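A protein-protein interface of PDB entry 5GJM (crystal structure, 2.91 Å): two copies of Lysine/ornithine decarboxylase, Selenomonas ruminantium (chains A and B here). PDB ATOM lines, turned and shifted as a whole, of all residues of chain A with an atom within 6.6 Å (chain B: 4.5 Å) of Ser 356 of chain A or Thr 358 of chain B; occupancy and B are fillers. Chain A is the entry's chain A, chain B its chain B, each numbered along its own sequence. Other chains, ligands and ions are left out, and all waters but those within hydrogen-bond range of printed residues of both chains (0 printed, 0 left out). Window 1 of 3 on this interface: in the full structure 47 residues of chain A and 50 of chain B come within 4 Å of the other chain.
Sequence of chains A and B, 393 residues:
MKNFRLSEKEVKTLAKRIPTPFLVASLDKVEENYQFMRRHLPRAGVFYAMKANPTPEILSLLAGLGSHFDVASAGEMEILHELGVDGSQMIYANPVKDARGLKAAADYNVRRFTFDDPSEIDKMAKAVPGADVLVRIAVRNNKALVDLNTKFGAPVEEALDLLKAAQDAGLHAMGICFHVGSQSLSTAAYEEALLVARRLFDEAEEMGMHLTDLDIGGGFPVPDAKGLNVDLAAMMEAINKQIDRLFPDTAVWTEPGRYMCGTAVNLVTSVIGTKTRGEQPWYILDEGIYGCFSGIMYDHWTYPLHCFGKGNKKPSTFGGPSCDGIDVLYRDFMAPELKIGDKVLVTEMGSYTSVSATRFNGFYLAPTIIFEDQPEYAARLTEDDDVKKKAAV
Of the printed residues of chain B, Ser 356 of chain A touches Thr 358 (3.2 Å). Thr 358 of chain B touches just these residues of chain A: Val 355 (3.8 Å), Ser 356 (3.2 Å), Ala 357 (3.5 Å) and Thr 358 (3.4 Å). Printed residues of chain B within 4 Å of Tyr 290 of chain A: Ser 356 (3.9 Å). Printed residues of chain B within 4 Å of Ala 357 of chain A: Thr 358. Printed residues of chain A within 4 Å of Ala 357 of chain B: Thr 358. Of the printed residues of chain A, Tyr 290 of chain B touches Tyr 298. Of the printed residues of chain B, Tyr 298 of chain A touches Tyr 290 (3.7 Å). Gly 295 of chain A touches none of the printed residues of chain B. The nearest residue of chain A that does not touch Thr 358 of chain B is Tyr 298 of chain A (5.6 Å). The nearest printed residue of chain B that does not touch Tyr 290 of chain A is Thr 358 of chain B (6.3 Å).
Tyr 290 of chain A touches Ser 356 of chain B. CD1 of Tyr 298 of chain A touches CE1 of Tyr 290 of chain B, at 3.7 Å. Val 355 of chain A touches Thr 358 of chain B (O to OG1, 3.8 Å). Val 355 of chain A touches Phe 360 of chain B. O of Ser 356 of chain A touches CG2 of Thr 358 of chain B, at 3.2 Å. O of Ala 357 of chain A touches CG2 of Thr 358 of chain B (3.5 Å). O of Ser 356 of chain B touches CG2 of Thr 358 of chain A, at 3.6 Å. Ala 357 of chain B touches Thr 358 of chain A (O to CB, 3.9 Å). CG2 of Thr 358 of chain B touches CG2 of Thr 358 of chain A (3.4 Å).
The backbone carbonyl oxygen (O) of Tyr 290 of chain B is in hydrogen-bond range of the backbone NH (N) of Thr 358 of chain B (2.7 Å). N of Thr 358 of chain A sits at hydrogen-bond distance from O of Tyr 290 of chain A (2.8 Å). O of Thr 353 of chain A sits at hydrogen-bond distance from OG of Ser 356 of chain A, 3.0 Å away. The backbone NH of Phe 360 of chain B sits close to the side-chain hydroxyl of Thr 358 of chain B, 3.4 Å away. The side-chain hydroxyl (OG) of Ser 356 of chain A lies within hydrogen-bond range of the side-chain hydroxyl (OG) of Ser 294 of chain A, at 2.7 Å.
Of the 15 printed residues of chain A, 6 touch a printed residue of chain B. Printed residues of chain B that touch a printed residue of chain A: Tyr 290, Ser 356, Ala 357, Thr 358 and Phe 360. Hydrophobic or aromatic side chains of chain B that line the printed part of chain A: Tyr 290 and Phe 360. Among the printed residues, 9 pairs touch across the chains. Among the printed residues, no Asp or Glu carboxylate lies within 4 Å of a Lys or Arg side-chain nitrogen of the other chain.
Tyr 290 of chain A touches Ser 356 of chain B, but with the chains exchanged Ser 356 of chain A does not touch Tyr 290 of chain B (4.4 Å). Ser 356 of chain A touches Thr 358 of chain B, and with the chains exchanged Thr 358 of chain A touches Ser 356 of chain B. Ala 357 of chain A touches Thr 358 of chain B, and with the chains exchanged Thr 358 of chain A touches Ala 357 of chain B. Thr 358 of chain B touches its own counterpart, Thr 358 of chain A. Positions printed for both chains: 290, 291, 356, 357 and 358. Of the 9 pairs that touch across the chains among the printed residues, 5 have their exchanged pair printed and touching as well.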
ATOM      1  N   ILE A 289     -35.161  16.692  33.361  1.00  0.00           N
ATOM      2  CA  ILE A 289     -34.423  15.991  32.324  1.00  0.00           C
ATOM      3  C   ILE A 289     -34.183  16.909  31.091  1.00  0.00           C
ATOM      4  O   ILE A 289     -33.226  16.733  30.360  1.00  0.00           O
ATOM      5  CB  ILE A 289     -35.188  14.684  31.972  1.00  0.00           C
ATOM      6  CG1 ILE A 289     -34.282  13.632  31.342  1.00  0.00           C
ATOM      7  CG2 ILE A 289     -36.364  14.947  31.039  1.00  0.00           C
ATOM      8  CD1 ILE A 289     -33.577  12.741  32.337  1.00  0.00           C
ATOM      9  N   TYR A 290     -35.050  17.894  30.879  1.00  0.00           N
ATOM     10  CA  TYR A 290     -34.853  18.901  29.837  1.00  0.00           C
ATOM     11  C   TYR A 290     -33.934  20.048  30.249  1.00  0.00           C
ATOM     12  O   TYR A 290     -33.636  20.919  29.423  1.00  0.00           O
ATOM     13  CB  TYR A 290     -36.191  19.480  29.424  1.00  0.00           C
ATOM     14  CG  TYR A 290     -37.089  18.487  28.698  1.00  0.00           C
ATOM     15  CD1 TYR A 290     -36.993  18.304  27.309  1.00  0.00           C
ATOM     16  CD2 TYR A 290     -38.048  17.762  29.388  1.00  0.00           C
ATOM     17  CE1 TYR A 290     -37.821  17.430  26.650  1.00  0.00           C
ATOM     18  CE2 TYR A 290     -38.880  16.874  28.735  1.00  0.00           C
ATOM     19  CZ  TYR A 290     -38.764  16.710  27.363  1.00  0.00           C
ATOM     20  OH  TYR A 290     -39.612  15.827  26.719  1.00  0.00           O
ATOM     21  N   GLY A 291     -33.508  20.057  31.515  1.00  0.00           N
ATOM     22  CA  GLY A 291     -32.613  21.068  32.056  1.00  0.00           C
ATOM     23  C   GLY A 291     -31.227  20.491  32.329  1.00  0.00           C
ATOM     24  O   GLY A 291     -30.597  19.913  31.436  1.00  0.00           O
ATOM     25  N   CYS A 292     -30.745  20.641  33.551  1.00  0.00           N
ATOM     26  CA  CYS A 292     -29.409  20.244  33.878  1.00  0.00           C
ATOM     27  C   CYS A 292     -29.247  18.755  34.063  1.00  0.00           C
ATOM     28  O   CYS A 292     -28.133  18.226  33.952  1.00  0.00           O
ATOM     29  CB  CYS A 292     -28.995  20.917  35.164  1.00  0.00           C
ATOM     30  SG  CYS A 292     -28.871  22.696  35.067  1.00  0.00           S
ATOM     31  N   PHE A 293     -30.342  18.084  34.404  1.00  0.00           N
ATOM     32  CA  PHE A 293     -30.345  16.633  34.536  1.00  0.00           C
ATOM     33  C   PHE A 293     -30.329  15.965  33.171  1.00  0.00           C
ATOM     34  O   PHE A 293     -30.314  14.768  33.091  1.00  0.00           O
ATOM     35  CB  PHE A 293     -31.563  16.168  35.332  1.00  0.00           C
ATOM     36  CG  PHE A 293     -31.524  16.521  36.794  1.00  0.00           C
ATOM     37  CD1 PHE A 293     -30.632  15.883  37.653  1.00  0.00           C
ATOM     38  CD2 PHE A 293     -32.423  17.426  37.327  1.00  0.00           C
ATOM     39  CE1 PHE A 293     -30.616  16.175  39.014  1.00  0.00           C
ATOM     40  CE2 PHE A 293     -32.416  17.720  38.683  1.00  0.00           C
ATOM     41  CZ  PHE A 293     -31.508  17.094  39.532  1.00  0.00           C
ATOM     42  N   SER A 294     -30.344  16.741  32.093  1.00  0.00           N
ATOM     43  CA  SER A 294     -30.156  16.247  30.723  1.00  0.00           C
ATOM     44  C   SER A 294     -28.986  15.287  30.560  1.00  0.00           C
ATOM     45  O   SER A 294     -29.015  14.428  29.670  1.00  0.00           O
ATOM     46  CB  SER A 294     -29.936  17.435  29.791  1.00  0.00           C
ATOM     47  OG  SER A 294     -28.883  18.259  30.274  1.00  0.00           O
ATOM     48  N   GLY A 295     -27.955  15.445  31.394  1.00  0.00           N
ATOM     49  CA  GLY A 295     -26.867  14.494  31.462  1.00  0.00           C
ATOM     50  C   GLY A 295     -27.233  13.066  31.841  1.00  0.00           C
ATOM     51  O   GLY A 295     -26.437  12.162  31.615  1.00  0.00           O
ATOM     52  N   TYR A 298     -28.116  12.265  28.115  1.00  0.00           N
ATOM     53  CA  TYR A 298     -27.041  12.373  27.119  1.00  0.00           C
ATOM     54  C   TYR A 298     -25.675  11.771  27.528  1.00  0.00           C
ATOM     55  O   TYR A 298     -24.932  11.259  26.669  1.00  0.00           O
ATOM     56  CB  TYR A 298     -26.878  13.828  26.702  1.00  0.00           C
ATOM     57  CG  TYR A 298     -27.967  14.343  25.799  1.00  0.00           C
ATOM     58  CD1 TYR A 298     -28.089  13.872  24.510  1.00  0.00           C
ATOM     59  CD2 TYR A 298     -28.853  15.338  26.212  1.00  0.00           C
ATOM     60  CE1 TYR A 298     -29.063  14.356  23.652  1.00  0.00           C
ATOM     61  CE2 TYR A 298     -29.831  15.828  25.353  1.00  0.00           C
ATOM     62  CZ  TYR A 298     -29.923  15.327  24.070  1.00  0.00           C
ATOM     63  OH  TYR A 298     -30.853  15.784  23.173  1.00  0.00           O
ATOM     64  N   TYR A 352     -21.078  18.849  31.477  1.00  0.00           N
ATOM     65  CA  TYR A 352     -21.972  18.178  30.558  1.00  0.00           C
ATOM     66  C   TYR A 352     -23.351  18.110  31.145  1.00  0.00           C
ATOM     67  O   TYR A 352     -24.023  17.113  31.074  1.00  0.00           O
ATOM     68  CB  TYR A 352     -21.442  16.803  30.198  1.00  0.00           C
ATOM     69  CG  TYR A 352     -20.127  16.852  29.499  1.00  0.00           C
ATOM     70  CD1 TYR A 352     -19.997  17.453  28.282  1.00  0.00           C
ATOM     71  CD2 TYR A 352     -19.012  16.307  30.068  1.00  0.00           C
ATOM     72  CE1 TYR A 352     -18.788  17.508  27.650  1.00  0.00           C
ATOM     73  CE2 TYR A 352     -17.807  16.357  29.440  1.00  0.00           C
ATOM     74  CZ  TYR A 352     -17.706  16.963  28.237  1.00  0.00           C
ATOM     75  OH  TYR A 352     -16.497  17.002  27.637  1.00  0.00           O
ATOM     76  N   THR A 353     -23.732  19.225  31.728  1.00  0.00           N
ATOM     77  CA  THR A 353     -24.943  19.383  32.476  1.00  0.00           C
ATOM     78  C   THR A 353     -25.786  20.489  31.821  1.00  0.00           C
ATOM     79  O   THR A 353     -26.653  20.212  31.040  1.00  0.00           O
ATOM     80  CB  THR A 353     -24.574  19.582  33.977  1.00  0.00           C
ATOM     81  OG1 THR A 353     -24.876  18.403  34.707  1.00  0.00           O
ATOM     82  CG2 THR A 353     -25.259  20.697  34.618  1.00  0.00           C
ATOM     83  N   SER A 354     -25.499  21.737  32.115  1.00  0.00           N
ATOM     84  CA  SER A 354     -26.261  22.853  31.612  1.00  0.00           C
ATOM     85  C   SER A 354     -26.109  23.051  30.122  1.00  0.00           C
ATOM     86  O   SER A 354     -26.919  23.658  29.481  1.00  0.00           O
ATOM     87  CB  SER A 354     -25.910  24.114  32.368  1.00  0.00           C
ATOM     88  OG  SER A 354     -24.625  24.547  32.040  1.00  0.00           O
ATOM     89  N   VAL A 355     -25.008  22.580  29.595  1.00  0.00           N
ATOM     90  CA  VAL A 355     -24.677  22.736  28.213  1.00  0.00           C
ATOM     91  C   VAL A 355     -25.722  22.090  27.317  1.00  0.00           C
ATOM     92  O   VAL A 355     -25.943  22.508  26.209  1.00  0.00           O
ATOM     93  CB  VAL A 355     -23.272  22.205  27.965  1.00  0.00           C
ATOM     94  CG1 VAL A 355     -22.295  23.090  28.687  1.00  0.00           C
ATOM     95  CG2 VAL A 355     -23.136  20.785  28.456  1.00  0.00           C
ATOM     96  N   SER A 356     -26.330  21.036  27.808  1.00  0.00           N
ATOM     97  CA  SER A 356     -27.352  20.328  27.091  1.00  0.00           C
ATOM     98  C   SER A 356     -28.763  20.722  27.504  1.00  0.00           C
ATOM     99  O   SER A 356     -29.699  20.072  27.135  1.00  0.00           O
ATOM    100  CB  SER A 356     -27.149  18.829  27.263  1.00  0.00           C
ATOM    101  OG  SER A 356     -26.826  18.497  28.590  1.00  0.00           O
ATOM    102  N   ALA A 357     -28.904  21.753  28.314  1.00  0.00           N
ATOM    103  CA  ALA A 357     -30.189  22.202  28.809  1.00  0.00           C
ATOM    104  C   ALA A 357     -31.012  22.949  27.779  1.00  0.00           C
ATOM    105  O   ALA A 357     -30.471  23.545  26.870  1.00  0.00           O
ATOM    106  CB  ALA A 357     -30.007  23.028  30.057  1.00  0.00           C
ATOM    107  N   THR A 358     -32.328  22.917  27.938  1.00  0.00           N
ATOM    108  CA  THR A 358     -33.230  23.469  26.933  1.00  0.00           C
ATOM    109  C   THR A 358     -34.281  24.404  27.553  1.00  0.00           C
ATOM    110  O   THR A 358     -34.462  24.469  28.769  1.00  0.00           O
ATOM    111  CB  THR A 358     -33.970  22.340  26.148  1.00  0.00           C
ATOM    112  OG1 THR A 358     -35.143  21.925  26.865  1.00  0.00           O
ATOM    113  CG2 THR A 358     -33.088  21.112  25.922  1.00  0.00           C
ATOM    114  N   TYR B 290     -28.235  16.916  19.638  1.00  0.00           N
ATOM    115  CA  TYR B 290     -28.239  18.096  20.511  1.00  0.00           C
ATOM    116  C   TYR B 290     -29.019  19.317  19.930  1.00  0.00           C
ATOM    117  O   TYR B 290     -29.191  20.352  20.608  1.00  0.00           O
ATOM    118  CB  TYR B 290     -26.784  18.483  20.829  1.00  0.00           C
ATOM    119  CG  TYR B 290     -26.049  17.474  21.676  1.00  0.00           C
ATOM    120  CD1 TYR B 290     -26.300  17.401  23.033  1.00  0.00           C
ATOM    121  CD2 TYR B 290     -25.112  16.620  21.133  1.00  0.00           C
ATOM    122  CE1 TYR B 290     -25.643  16.500  23.845  1.00  0.00           C
ATOM    123  CE2 TYR B 290     -24.440  15.710  21.927  1.00  0.00           C
ATOM    124  CZ  TYR B 290     -24.709  15.648  23.295  1.00  0.00           C
ATOM    125  OH  TYR B 290     -24.069  14.757  24.138  1.00  0.00           O
ATOM    126  N   GLY B 291     -29.461  19.198  18.676  1.00  0.00           N
ATOM    127  CA  GLY B 291     -30.253  20.218  18.014  1.00  0.00           C
ATOM    128  C   GLY B 291     -31.623  19.622  17.763  1.00  0.00           C
ATOM    129  O   GLY B 291     -32.333  19.257  18.683  1.00  0.00           O
ATOM    130  N   SER B 356     -36.498  21.021  21.999  1.00  0.00           N
ATOM    131  CA  SER B 356     -35.494  20.319  22.752  1.00  0.00           C
ATOM    132  C   SER B 356     -34.088  20.614  22.293  1.00  0.00           C
ATOM    133  O   SER B 356     -33.195  19.874  22.596  1.00  0.00           O
ATOM    134  CB  SER B 356     -35.705  18.831  22.620  1.00  0.00           C
ATOM    135  OG  SER B 356     -36.991  18.456  22.987  1.00  0.00           O
ATOM    136  N   ALA B 357     -33.883  21.630  21.477  1.00  0.00           N
ATOM    137  CA  ALA B 357     -32.536  21.854  20.931  1.00  0.00           C
ATOM    138  C   ALA B 357     -31.693  22.640  21.907  1.00  0.00           C
ATOM    139  O   ALA B 357     -32.211  23.327  22.795  1.00  0.00           O
ATOM    140  CB  ALA B 357     -32.584  22.539  19.580  1.00  0.00           C
ATOM    141  N   THR B 358     -30.387  22.520  21.741  1.00  0.00           N
ATOM    142  CA  THR B 358     -29.420  23.116  22.638  1.00  0.00           C
ATOM    143  C   THR B 358     -28.228  23.731  21.893  1.00  0.00           C
ATOM    144  O   THR B 358     -28.045  23.523  20.708  1.00  0.00           O
ATOM    145  CB  THR B 358     -28.987  22.133  23.739  1.00  0.00           C
ATOM    146  OG1 THR B 358     -27.988  21.251  23.255  1.00  0.00           O
ATOM    147  CG2 THR B 358     -30.127  21.321  24.180  1.00  0.00           C
ATOM    148  N   ARG B 359     -27.411  24.472  22.614  1.00  0.00           N
ATOM    149  CA  ARG B 359     -26.223  25.095  22.073  1.00  0.00           C
ATOM    150  C   ARG B 359     -25.013  24.338  22.530  1.00  0.00           C
ATOM    151  O   ARG B 359     -24.003  24.895  22.810  1.00  0.00           O
ATOM    152  CB  ARG B 359     -26.119  26.564  22.435  1.00  0.00           C
ATOM    153  CG  ARG B 359     -27.347  27.358  22.068  1.00  0.00           C
ATOM    154  CD  ARG B 359     -27.086  28.507  21.124  1.00  0.00           C
ATOM    155  NE  ARG B 359     -25.742  28.581  20.578  1.00  0.00           N
ATOM    156  CZ  ARG B 359     -24.943  29.623  20.732  1.00  0.00           C
ATOM    157  NH1 ARG B 359     -25.342  30.656  21.433  1.00  0.00           N
ATOM    158  NH2 ARG B 359     -23.747  29.626  20.200  1.00  0.00           N
ATOM    159  N   PHE B 360     -25.175  23.047  22.657  1.00  0.00           N
ATOM    160  CA  PHE B 360     -24.128  22.177  23.067  1.00  0.00           C
ATOM    161  C   PHE B 360     -23.017  22.238  22.067  1.00  0.00           C
ATOM    162  O   PHE B 360     -23.252  22.216  20.891  1.00  0.00           O
ATOM    163  CB  PHE B 360     -24.677  20.762  23.152  1.00  0.00           C
ATOM    164  CG  PHE B 360     -23.684  19.761  23.618  1.00  0.00           C
ATOM    165  CD1 PHE B 360     -23.421  19.618  24.939  1.00  0.00           C
ATOM    166  CD2 PHE B 360     -23.003  18.976  22.722  1.00  0.00           C
ATOM    167  CE1 PHE B 360     -22.500  18.710  25.370  1.00  0.00           C
ATOM    168  CE2 PHE B 360     -22.072  18.069  23.142  1.00  0.00           C
ATOM    169  CZ  PHE B 360     -21.820  17.939  24.468  1.00  0.00           C
ATOM    170  N   PHE B 363     -22.815  25.332  19.381  1.00  0.00           N
ATOM    171  CA  PHE B 363     -23.524  25.378  18.129  1.00  0.00           C
ATOM    172  C   PHE B 363     -24.750  26.255  18.209  1.00  0.00           C
ATOM    173  O   PHE B 363     -25.338  26.384  19.250  1.00  0.00           O
ATOM    174  CB  PHE B 363     -23.911  23.966  17.718  1.00  0.00           C
ATOM    175  CG  PHE B 363     -22.816  23.198  17.042  1.00  0.00           C
ATOM    176  CD1 PHE B 363     -22.417  23.513  15.777  1.00  0.00           C
ATOM    177  CD2 PHE B 363     -22.211  22.145  17.665  1.00  0.00           C
ATOM    178  CE1 PHE B 363     -21.423  22.797  15.147  1.00  0.00           C
ATOM    179  CE2 PHE B 363     -21.219  21.434  17.052  1.00  0.00           C
ATOM    180  CZ  PHE B 363     -20.827  21.758  15.790  1.00  0.00           C
ATOM    181  N   LEU B 365     -28.691  27.435  17.322  1.00  0.00           N
ATOM    182  CA  LEU B 365     -30.002  26.797  17.165  1.00  0.00           C
ATOM    183  C   LEU B 365     -30.364  26.973  15.719  1.00  0.00           C
ATOM    184  O   LEU B 365     -30.197  28.077  15.203  1.00  0.00           O
ATOM    185  CB  LEU B 365     -31.073  27.489  18.026  1.00  0.00           C
ATOM    186  CG  LEU B 365     -30.770  27.479  19.532  1.00  0.00           C
ATOM    187  CD1 LEU B 365     -31.749  28.358  20.294  1.00  0.00           C
ATOM    188  CD2 LEU B 365     -30.739  26.028  20.055  1.00  0.00           C
